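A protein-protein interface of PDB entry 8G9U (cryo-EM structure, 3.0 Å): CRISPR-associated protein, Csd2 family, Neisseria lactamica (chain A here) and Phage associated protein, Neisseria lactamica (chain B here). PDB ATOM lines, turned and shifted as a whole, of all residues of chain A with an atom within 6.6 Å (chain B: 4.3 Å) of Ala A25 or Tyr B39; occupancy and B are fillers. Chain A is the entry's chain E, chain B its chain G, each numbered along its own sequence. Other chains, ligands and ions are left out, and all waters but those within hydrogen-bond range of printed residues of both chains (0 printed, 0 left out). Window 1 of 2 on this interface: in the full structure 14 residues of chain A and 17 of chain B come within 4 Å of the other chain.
The backbone carbonyl oxygen (O) of Pro A23 lies close to the backbone carbonyl oxygen (O) of Arg B38, at 3.3 Å.
O of Tyr B39 sits close to O of Asp A24 (2.8 Å).
The backbone carbonyl oxygen (O) of Asp A24 is in hydrogen-bond range of the backbone NH (N) of Gly B41 (3.5 Å).
N of Gly A26 sits at hydrogen-bond distance from O of Arg B38 (2.7 Å).
NE of Arg A168 lies within hydrogen-bond range of OH of Tyr B39 (3.5 Å).
The backbone carbonyl oxygen of Asp A24 lies within hydrogen-bond range of the side-chain hydroxyl of Ser B42, 2.8 Å away.
The backbone carbonyl oxygen of Arg B38 lies close to the backbone carbonyl oxygen of Asp A24, at 3.4 Å.
OD1 of Asp A22 sits close to N of Asp A24, 3.5 Å away.
The backbone NH of Asp A22 is in hydrogen-bond range of the backbone carbonyl oxygen of Leu A28, at 2.4 Å.
The backbone carbonyl oxygen of Val B50 sits at hydrogen-bond distance from the side-chain hydroxyl of Thr B53, at 2.8 Å.
O of Tyr B39 lies within hydrogen-bond range of OG of Ser B42, 3.2 Å away.
C of Ala A25 touches O of Arg B38 (3.7 Å).
CD1 of Tyr B39 touches C of Ala A25, at 3.96 Å.
Ala A25 touches Ser B42.
Ala A25 touches Val B50.
CD1 of Tyr B39 touches N of Gly A26, 3.1 Å away.
Leu A28 touches Thr B53.
CG of Glu A143 touches CG2 of Thr B53, at 3.7 Å.
Arg A168 touches Leu B57.
OH of Tyr B39 touches CZ of Phe A170 (3.2 Å).
Ala A25 touches four residues of chain B.
Of chain A, only Asp A24, Ala A25, Gly A26, Arg A168 and Phe A170 come within 4 Å of Tyr B39.
Of the printed residues of chain B, Pro A23 touches Arg B38.
Of the printed residues of chain A, Leu B57 touches Arg A168.
Of the printed residues of chain B, Leu A28 touches Thr B53 (3.8 Å).
Leu B54 touches none of the printed residues of chain A.
The nearest printed residue of chain B that does not touch Ala A25 is Gly B41 (5.4 Å).
The nearest residue of chain A that does not touch Tyr B39 is Leu A28 (5.0 Å).
Of the 14 printed residues of chain B, 7 touch a printed residue of chain A.
Hydrophobic or aromatic side chains of chain B within 4 Å of the printed part of chain A: Tyr B39, Val B50 and Leu B57.
Printed residues of chain A that touch a printed residue of chain B: Pro A23, Asp A24, Ala A25, Gly A26, Leu A28, Glu A143, Arg A168 and Phe A170.
Hydrophobic or aromatic side chains of chain A within 4 Å of the printed part of chain B: Ala A25, Leu A28 and Phe A170.
Among the printed residues, 16 pairs touch across the chains.
Among the printed residues, no Asp or Glu carboxylate lies within 4 Å of a Lys or Arg side-chain nitrogen of the other chain.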
ATOM      1  N   GLY A  21      23.725   4.833   4.979  1.00  0.00           N
ATOM      2  CA  GLY A  21      24.048   3.587   5.631  1.00  0.00           C
ATOM      3  C   GLY A  21      24.591   3.818   7.025  1.00  0.00           C
ATOM      4  O   GLY A  21      25.249   4.816   7.301  1.00  0.00           O
ATOM      5  N   ASP A  22      24.299   2.888   7.918  1.00  0.00           N
ATOM      6  CA  ASP A  22      24.821   2.962   9.269  1.00  0.00           C
ATOM      7  C   ASP A  22      26.115   2.175   9.303  1.00  0.00           C
ATOM      8  O   ASP A  22      26.082   0.951   9.135  1.00  0.00           O
ATOM      9  CB  ASP A  22      23.824   2.392  10.262  1.00  0.00           C
ATOM     10  CG  ASP A  22      24.056   2.886  11.672  1.00  0.00           C
ATOM     11  OD1 ASP A  22      25.051   3.599  11.899  1.00  0.00           O
ATOM     12  OD2 ASP A  22      23.240   2.564  12.558  1.00  0.00           O
ATOM     13  N   PRO A  23      27.265   2.811   9.494  1.00  0.00           N
ATOM     14  CA  PRO A  23      28.505   2.036   9.600  1.00  0.00           C
ATOM     15  C   PRO A  23      28.501   1.080  10.765  1.00  0.00           C
ATOM     16  O   PRO A  23      29.243   0.092  10.756  1.00  0.00           O
ATOM     17  CB  PRO A  23      29.580   3.111   9.761  1.00  0.00           C
ATOM     18  CG  PRO A  23      28.969   4.353   9.336  1.00  0.00           C
ATOM     19  CD  PRO A  23      27.507   4.254   9.514  1.00  0.00           C
ATOM     20  N   ASP A  24      27.696   1.355  11.784  1.00  0.00           N
ATOM     21  CA  ASP A  24      27.492   0.392  12.847  1.00  0.00           C
ATOM     22  C   ASP A  24      26.639  -0.782  12.396  1.00  0.00           C
ATOM     23  O   ASP A  24      26.664  -1.833  13.041  1.00  0.00           O
ATOM     24  CB  ASP A  24      26.837   1.080  14.037  1.00  0.00           C
ATOM     25  CG  ASP A  24      27.812   1.910  14.831  1.00  0.00           C
ATOM     26  OD1 ASP A  24      29.030   1.778  14.586  1.00  0.00           O
ATOM     27  OD2 ASP A  24      27.364   2.691  15.698  1.00  0.00           O
ATOM     28  N   ALA A  25      25.890  -0.634  11.307  1.00  0.00           N
ATOM     29  CA  ALA A  25      25.042  -1.700  10.775  1.00  0.00           C
ATOM     30  C   ALA A  25      25.385  -1.860   9.307  1.00  0.00           C
ATOM     31  O   ALA A  25      24.690  -1.335   8.439  1.00  0.00           O
ATOM     32  CB  ALA A  25      23.576  -1.374  10.967  1.00  0.00           C
ATOM     33  N   GLY A  26      26.444  -2.611   9.031  1.00  0.00           N
ATOM     34  CA  GLY A  26      26.863  -2.871   7.671  1.00  0.00           C
ATOM     35  C   GLY A  26      26.941  -1.624   6.838  1.00  0.00           C
ATOM     36  O   GLY A  26      27.762  -0.746   7.085  1.00  0.00           O
ATOM     37  N   ASN A  27      26.081  -1.555   5.835  1.00  0.00           N
ATOM     38  CA  ASN A  27      25.719  -0.290   5.220  1.00  0.00           C
ATOM     39  C   ASN A  27      24.222  -0.084   5.361  1.00  0.00           C
ATOM     40  O   ASN A  27      23.618   0.632   4.563  1.00  0.00           O
ATOM     41  CB  ASN A  27      26.149  -0.248   3.754  1.00  0.00           C
ATOM     42  CG  ASN A  27      26.263   1.154   3.226  1.00  0.00           C
ATOM     43  OD1 ASN A  27      26.506   2.083   3.985  1.00  0.00           O
ATOM     44  ND2 ASN A  27      26.113   1.316   1.920  1.00  0.00           N
ATOM     45  N   LEU A  28      23.619  -0.723   6.360  1.00  0.00           N
ATOM     46  CA  LEU A  28      22.174  -0.693   6.505  1.00  0.00           C
ATOM     47  C   LEU A  28      21.709   0.741   6.691  1.00  0.00           C
ATOM     48  O   LEU A  28      22.355   1.511   7.408  1.00  0.00           O
ATOM     49  CB  LEU A  28      21.730  -1.533   7.700  1.00  0.00           C
ATOM     50  CG  LEU A  28      21.398  -2.992   7.425  1.00  0.00           C
ATOM     51  CD1 LEU A  28      21.448  -3.780   8.705  1.00  0.00           C
ATOM     52  CD2 LEU A  28      20.027  -3.089   6.803  1.00  0.00           C
ATOM     53  N   PRO A  29      20.608   1.136   6.064  1.00  0.00           N
ATOM     54  CA  PRO A  29      20.110   2.492   6.264  1.00  0.00           C
ATOM     55  C   PRO A  29      19.929   2.752   7.745  1.00  0.00           C
ATOM     56  O   PRO A  29      19.447   1.895   8.485  1.00  0.00           O
ATOM     57  CB  PRO A  29      18.776   2.493   5.518  1.00  0.00           C
ATOM     58  CG  PRO A  29      18.883   1.383   4.556  1.00  0.00           C
ATOM     59  CD  PRO A  29      19.713   0.343   5.214  1.00  0.00           C
ATOM     60  N   GLU A 143      17.745  -5.211   2.318  1.00  0.00           N
ATOM     61  CA  GLU A 143      18.875  -6.119   2.442  1.00  0.00           C
ATOM     62  C   GLU A 143      18.951  -6.983   1.184  1.00  0.00           C
ATOM     63  O   GLU A 143      18.828  -8.203   1.216  1.00  0.00           O
ATOM     64  CB  GLU A 143      18.770  -6.930   3.744  1.00  0.00           C
ATOM     65  CG  GLU A 143      19.959  -7.785   4.193  1.00  0.00           C
ATOM     66  CD  GLU A 143      20.011  -9.165   3.560  1.00  0.00           C
ATOM     67  OE1 GLU A 143      18.936  -9.703   3.224  1.00  0.00           O
ATOM     68  OE2 GLU A 143      21.118  -9.722   3.412  1.00  0.00           O
ATOM     69  N   ARG A 168      26.033  -7.488   0.136  1.00  0.00           N
ATOM     70  CA  ARG A 168      24.701  -6.908   0.220  1.00  0.00           C
ATOM     71  C   ARG A 168      24.666  -5.477  -0.287  1.00  0.00           C
ATOM     72  O   ARG A 168      25.628  -4.725  -0.121  1.00  0.00           O
ATOM     73  CB  ARG A 168      24.204  -6.908   1.658  1.00  0.00           C
ATOM     74  CG  ARG A 168      23.602  -8.202   2.106  1.00  0.00           C
ATOM     75  CD  ARG A 168      23.922  -8.445   3.559  1.00  0.00           C
ATOM     76  NE  ARG A 168      25.359  -8.538   3.771  1.00  0.00           N
ATOM     77  CZ  ARG A 168      26.074  -9.623   3.506  1.00  0.00           C
ATOM     78  NH1 ARG A 168      27.379  -9.633   3.734  1.00  0.00           N
ATOM     79  NH2 ARG A 168      25.483 -10.691   2.988  1.00  0.00           N
ATOM     80  N   PHE A 170      21.975  -2.996   0.859  1.00  0.00           N
ATOM     81  CA  PHE A 170      20.802  -2.571   1.599  1.00  0.00           C
ATOM     82  C   PHE A 170      20.153  -1.402   0.880  1.00  0.00           C
ATOM     83  O   PHE A 170      20.839  -0.465   0.468  1.00  0.00           O
ATOM     84  CB  PHE A 170      21.219  -2.171   3.001  1.00  0.00           C
ATOM     85  CG  PHE A 170      22.058  -3.196   3.681  1.00  0.00           C
ATOM     86  CD1 PHE A 170      21.566  -4.454   3.929  1.00  0.00           C
ATOM     87  CD2 PHE A 170      23.362  -2.920   4.012  1.00  0.00           C
ATOM     88  CE1 PHE A 170      22.346  -5.401   4.546  1.00  0.00           C
ATOM     89  CE2 PHE A 170      24.147  -3.863   4.624  1.00  0.00           C
ATOM     90  CZ  PHE A 170      23.638  -5.107   4.890  1.00  0.00           C
ATOM     91  N   PHE B  17      25.514 -12.769  19.034  1.00  0.00           N
ATOM     92  CA  PHE B  17      26.437 -12.132  18.115  1.00  0.00           C
ATOM     93  C   PHE B  17      27.812 -12.757  18.210  1.00  0.00           C
ATOM     94  O   PHE B  17      28.527 -12.854  17.211  1.00  0.00           O
ATOM     95  CB  PHE B  17      26.514 -10.646  18.405  1.00  0.00           C
ATOM     96  CG  PHE B  17      27.239  -9.886  17.372  1.00  0.00           C
ATOM     97  CD1 PHE B  17      28.596  -9.724  17.454  1.00  0.00           C
ATOM     98  CD2 PHE B  17      26.571  -9.354  16.303  1.00  0.00           C
ATOM     99  CE1 PHE B  17      29.264  -9.041  16.500  1.00  0.00           C
ATOM    100  CE2 PHE B  17      27.238  -8.666  15.353  1.00  0.00           C
ATOM    101  CZ  PHE B  17      28.586  -8.510  15.452  1.00  0.00           C
ATOM    102  N   ILE B  35      31.620  -9.672  11.287  1.00  0.00           N
ATOM    103  CA  ILE B  35      30.422  -8.943  11.674  1.00  0.00           C
ATOM    104  C   ILE B  35      30.664  -8.128  12.931  1.00  0.00           C
ATOM    105  O   ILE B  35      29.922  -7.189  13.208  1.00  0.00           O
ATOM    106  CB  ILE B  35      29.228  -9.892  11.839  1.00  0.00           C
ATOM    107  CG1 ILE B  35      29.543 -10.937  12.887  1.00  0.00           C
ATOM    108  CG2 ILE B  35      28.857 -10.516  10.522  1.00  0.00           C
ATOM    109  CD1 ILE B  35      28.367 -11.732  13.262  1.00  0.00           C
ATOM    110  N   ALA B  36      31.696  -8.441  13.705  1.00  0.00           N
ATOM    111  CA  ALA B  36      32.096  -7.487  14.731  1.00  0.00           C
ATOM    112  C   ALA B  36      32.567  -6.193  14.092  1.00  0.00           C
ATOM    113  O   ALA B  36      32.254  -5.095  14.560  1.00  0.00           O
ATOM    114  CB  ALA B  36      33.190  -8.069  15.614  1.00  0.00           C
ATOM    115  N   ASP B  37      33.315  -6.304  13.005  1.00  0.00           N
ATOM    116  CA  ASP B  37      33.908  -5.140  12.375  1.00  0.00           C
ATOM    117  C   ASP B  37      32.915  -4.325  11.563  1.00  0.00           C
ATOM    118  O   ASP B  37      33.221  -3.172  11.239  1.00  0.00           O
ATOM    119  CB  ASP B  37      35.080  -5.612  11.529  1.00  0.00           C
ATOM    120  CG  ASP B  37      36.038  -6.464  12.330  1.00  0.00           C
ATOM    121  OD1 ASP B  37      36.354  -6.055  13.468  1.00  0.00           O
ATOM    122  OD2 ASP B  37      36.438  -7.560  11.874  1.00  0.00           O
ATOM    123  N   ARG B  38      31.734  -4.863  11.269  1.00  0.00           N
ATOM    124  CA  ARG B  38      30.782  -4.212  10.375  1.00  0.00           C
ATOM    125  C   ARG B  38      29.377  -4.089  10.956  1.00  0.00           C
ATOM    126  O   ARG B  38      28.643  -3.171  10.579  1.00  0.00           O
ATOM    127  CB  ARG B  38      30.752  -4.985   9.041  1.00  0.00           C
ATOM    128  CG  ARG B  38      29.407  -5.068   8.393  1.00  0.00           C
ATOM    129  CD  ARG B  38      29.329  -6.034   7.222  1.00  0.00           C
ATOM    130  NE  ARG B  38      30.339  -7.089   7.307  1.00  0.00           N
ATOM    131  CZ  ARG B  38      31.214  -7.371   6.345  1.00  0.00           C
ATOM    132  NH1 ARG B  38      31.189  -6.703   5.196  1.00  0.00           N
ATOM    133  NH2 ARG B  38      32.096  -8.345   6.518  1.00  0.00           N
ATOM    134  N   TYR B  39      28.996  -4.964  11.890  1.00  0.00           N
ATOM    135  CA  TYR B  39      27.643  -5.036  12.430  1.00  0.00           C
ATOM    136  C   TYR B  39      27.573  -4.755  13.922  1.00  0.00           C
ATOM    137  O   TYR B  39      26.521  -4.321  14.397  1.00  0.00           O
ATOM    138  CB  TYR B  39      27.047  -6.428  12.173  1.00  0.00           C
ATOM    139  CG  TYR B  39      26.492  -6.628  10.790  1.00  0.00           C
ATOM    140  CD1 TYR B  39      26.505  -5.620   9.876  1.00  0.00           C
ATOM    141  CD2 TYR B  39      25.987  -7.838  10.388  1.00  0.00           C
ATOM    142  CE1 TYR B  39      26.017  -5.804   8.608  1.00  0.00           C
ATOM    143  CE2 TYR B  39      25.493  -8.023   9.117  1.00  0.00           C
ATOM    144  CZ  TYR B  39      25.514  -6.997   8.231  1.00  0.00           C
ATOM    145  OH  TYR B  39      25.023  -7.164   6.952  1.00  0.00           O
ATOM    146  N   PHE B  40      28.661  -4.978  14.664  1.00  0.00           N
ATOM    147  CA  PHE B  40      28.610  -4.932  16.125  1.00  0.00           C
ATOM    148  C   PHE B  40      28.082  -3.597  16.625  1.00  0.00           C
ATOM    149  O   PHE B  40      27.347  -3.547  17.614  1.00  0.00           O
ATOM    150  CB  PHE B  40      29.997  -5.193  16.713  1.00  0.00           C
ATOM    151  CG  PHE B  40      29.995  -5.471  18.188  1.00  0.00           C
ATOM    152  CD1 PHE B  40      29.722  -4.483  19.100  1.00  0.00           C
ATOM    153  CD2 PHE B  40      30.318  -6.718  18.660  1.00  0.00           C
ATOM    154  CE1 PHE B  40      29.721  -4.745  20.435  1.00  0.00           C
ATOM    155  CE2 PHE B  40      30.328  -6.973  20.004  1.00  0.00           C
ATOM    156  CZ  PHE B  40      30.031  -5.982  20.889  1.00  0.00           C
ATOM    157  N   GLY B  41      28.439  -2.507  15.956  1.00  0.00           N
ATOM    158  CA  GLY B  41      28.058  -1.200  16.454  1.00  0.00           C
ATOM    159  C   GLY B  41      26.566  -1.063  16.671  1.00  0.00           C
ATOM    160  O   GLY B  41      26.126  -0.431  17.630  1.00  0.00           O
ATOM    161  N   SER B  42      25.768  -1.660  15.793  1.00  0.00           N
ATOM    162  CA  SER B  42      24.326  -1.603  15.966  1.00  0.00           C
ATOM    163  C   SER B  42      23.777  -2.867  16.594  1.00  0.00           C
ATOM    164  O   SER B  42      22.786  -2.806  17.322  1.00  0.00           O
ATOM    165  CB  SER B  42      23.643  -1.375  14.632  1.00  0.00           C
ATOM    166  OG  SER B  42      24.017  -2.411  13.762  1.00  0.00           O
ATOM    167  N   ALA B  43      24.401  -4.014  16.339  1.00  0.00           N
ATOM    168  CA  ALA B  43      23.991  -5.224  17.032  1.00  0.00           C
ATOM    169  C   ALA B  43      23.991  -5.007  18.527  1.00  0.00           C
ATOM    170  O   ALA B  43      23.113  -5.510  19.230  1.00  0.00           O
ATOM    171  CB  ALA B  43      24.916  -6.377  16.669  1.00  0.00           C
ATOM    172  N   VAL B  50      20.530  -5.144  12.478  1.00  0.00           N
ATOM    173  CA  VAL B  50      21.375  -6.187  11.939  1.00  0.00           C
ATOM    174  C   VAL B  50      20.781  -7.570  12.150  1.00  0.00           C
ATOM    175  O   VAL B  50      20.587  -8.297  11.181  1.00  0.00           O
ATOM    176  CB  VAL B  50      22.790  -6.088  12.532  1.00  0.00           C
ATOM    177  CG1 VAL B  50      23.459  -4.864  12.008  1.00  0.00           C
ATOM    178  CG2 VAL B  50      22.689  -5.975  14.000  1.00  0.00           C
ATOM    179  N   THR B  53      19.483  -9.280   9.464  1.00  0.00           N
ATOM    180  CA  THR B  53      20.425  -9.538   8.383  1.00  0.00           C
ATOM    181  C   THR B  53      21.517 -10.500   8.795  1.00  0.00           C
ATOM    182  O   THR B  53      22.022 -11.245   7.955  1.00  0.00           O
ATOM    183  CB  THR B  53      21.067  -8.245   7.930  1.00  0.00           C
ATOM    184  OG1 THR B  53      22.060  -7.869   8.884  1.00  0.00           O
ATOM    185  CG2 THR B  53      20.028  -7.172   7.890  1.00  0.00           C
ATOM    186  N   LEU B  54      21.893 -10.483  10.067  1.00  0.00           N
ATOM    187  CA  LEU B  54      22.868 -11.417  10.599  1.00  0.00           C
ATOM    188  C   LEU B  54      22.421 -12.850  10.434  1.00  0.00           C
ATOM    189  O   LEU B  54      23.244 -13.767  10.497  1.00  0.00           O
ATOM    190  CB  LEU B  54      23.106 -11.103  12.064  1.00  0.00           C
ATOM    191  CG  LEU B  54      24.153 -10.028  12.207  1.00  0.00           C
ATOM    192  CD1 LEU B  54      24.349  -9.665  13.636  1.00  0.00           C
ATOM    193  CD2 LEU B  54      25.383 -10.696  11.690  1.00  0.00           C
ATOM    194  N   LEU B  57      22.382 -14.006   6.861  1.00  0.00           N
ATOM    195  CA  LEU B  57      23.800 -14.182   6.636  1.00  0.00           C
ATOM    196  C   LEU B  57      24.345 -15.402   7.346  1.00  0.00           C
ATOM    197  O   LEU B  57      25.455 -15.846   7.044  1.00  0.00           O
ATOM    198  CB  LEU B  57      24.497 -12.915   7.130  1.00  0.00           C
ATOM    199  CG  LEU B  57      25.959 -12.594   6.970  1.00  0.00           C
ATOM    200  CD1 LEU B  57      26.183 -12.466   5.513  1.00  0.00           C
ATOM    201  CD2 LEU B  57      26.282 -11.296   7.673  1.00  0.00           C
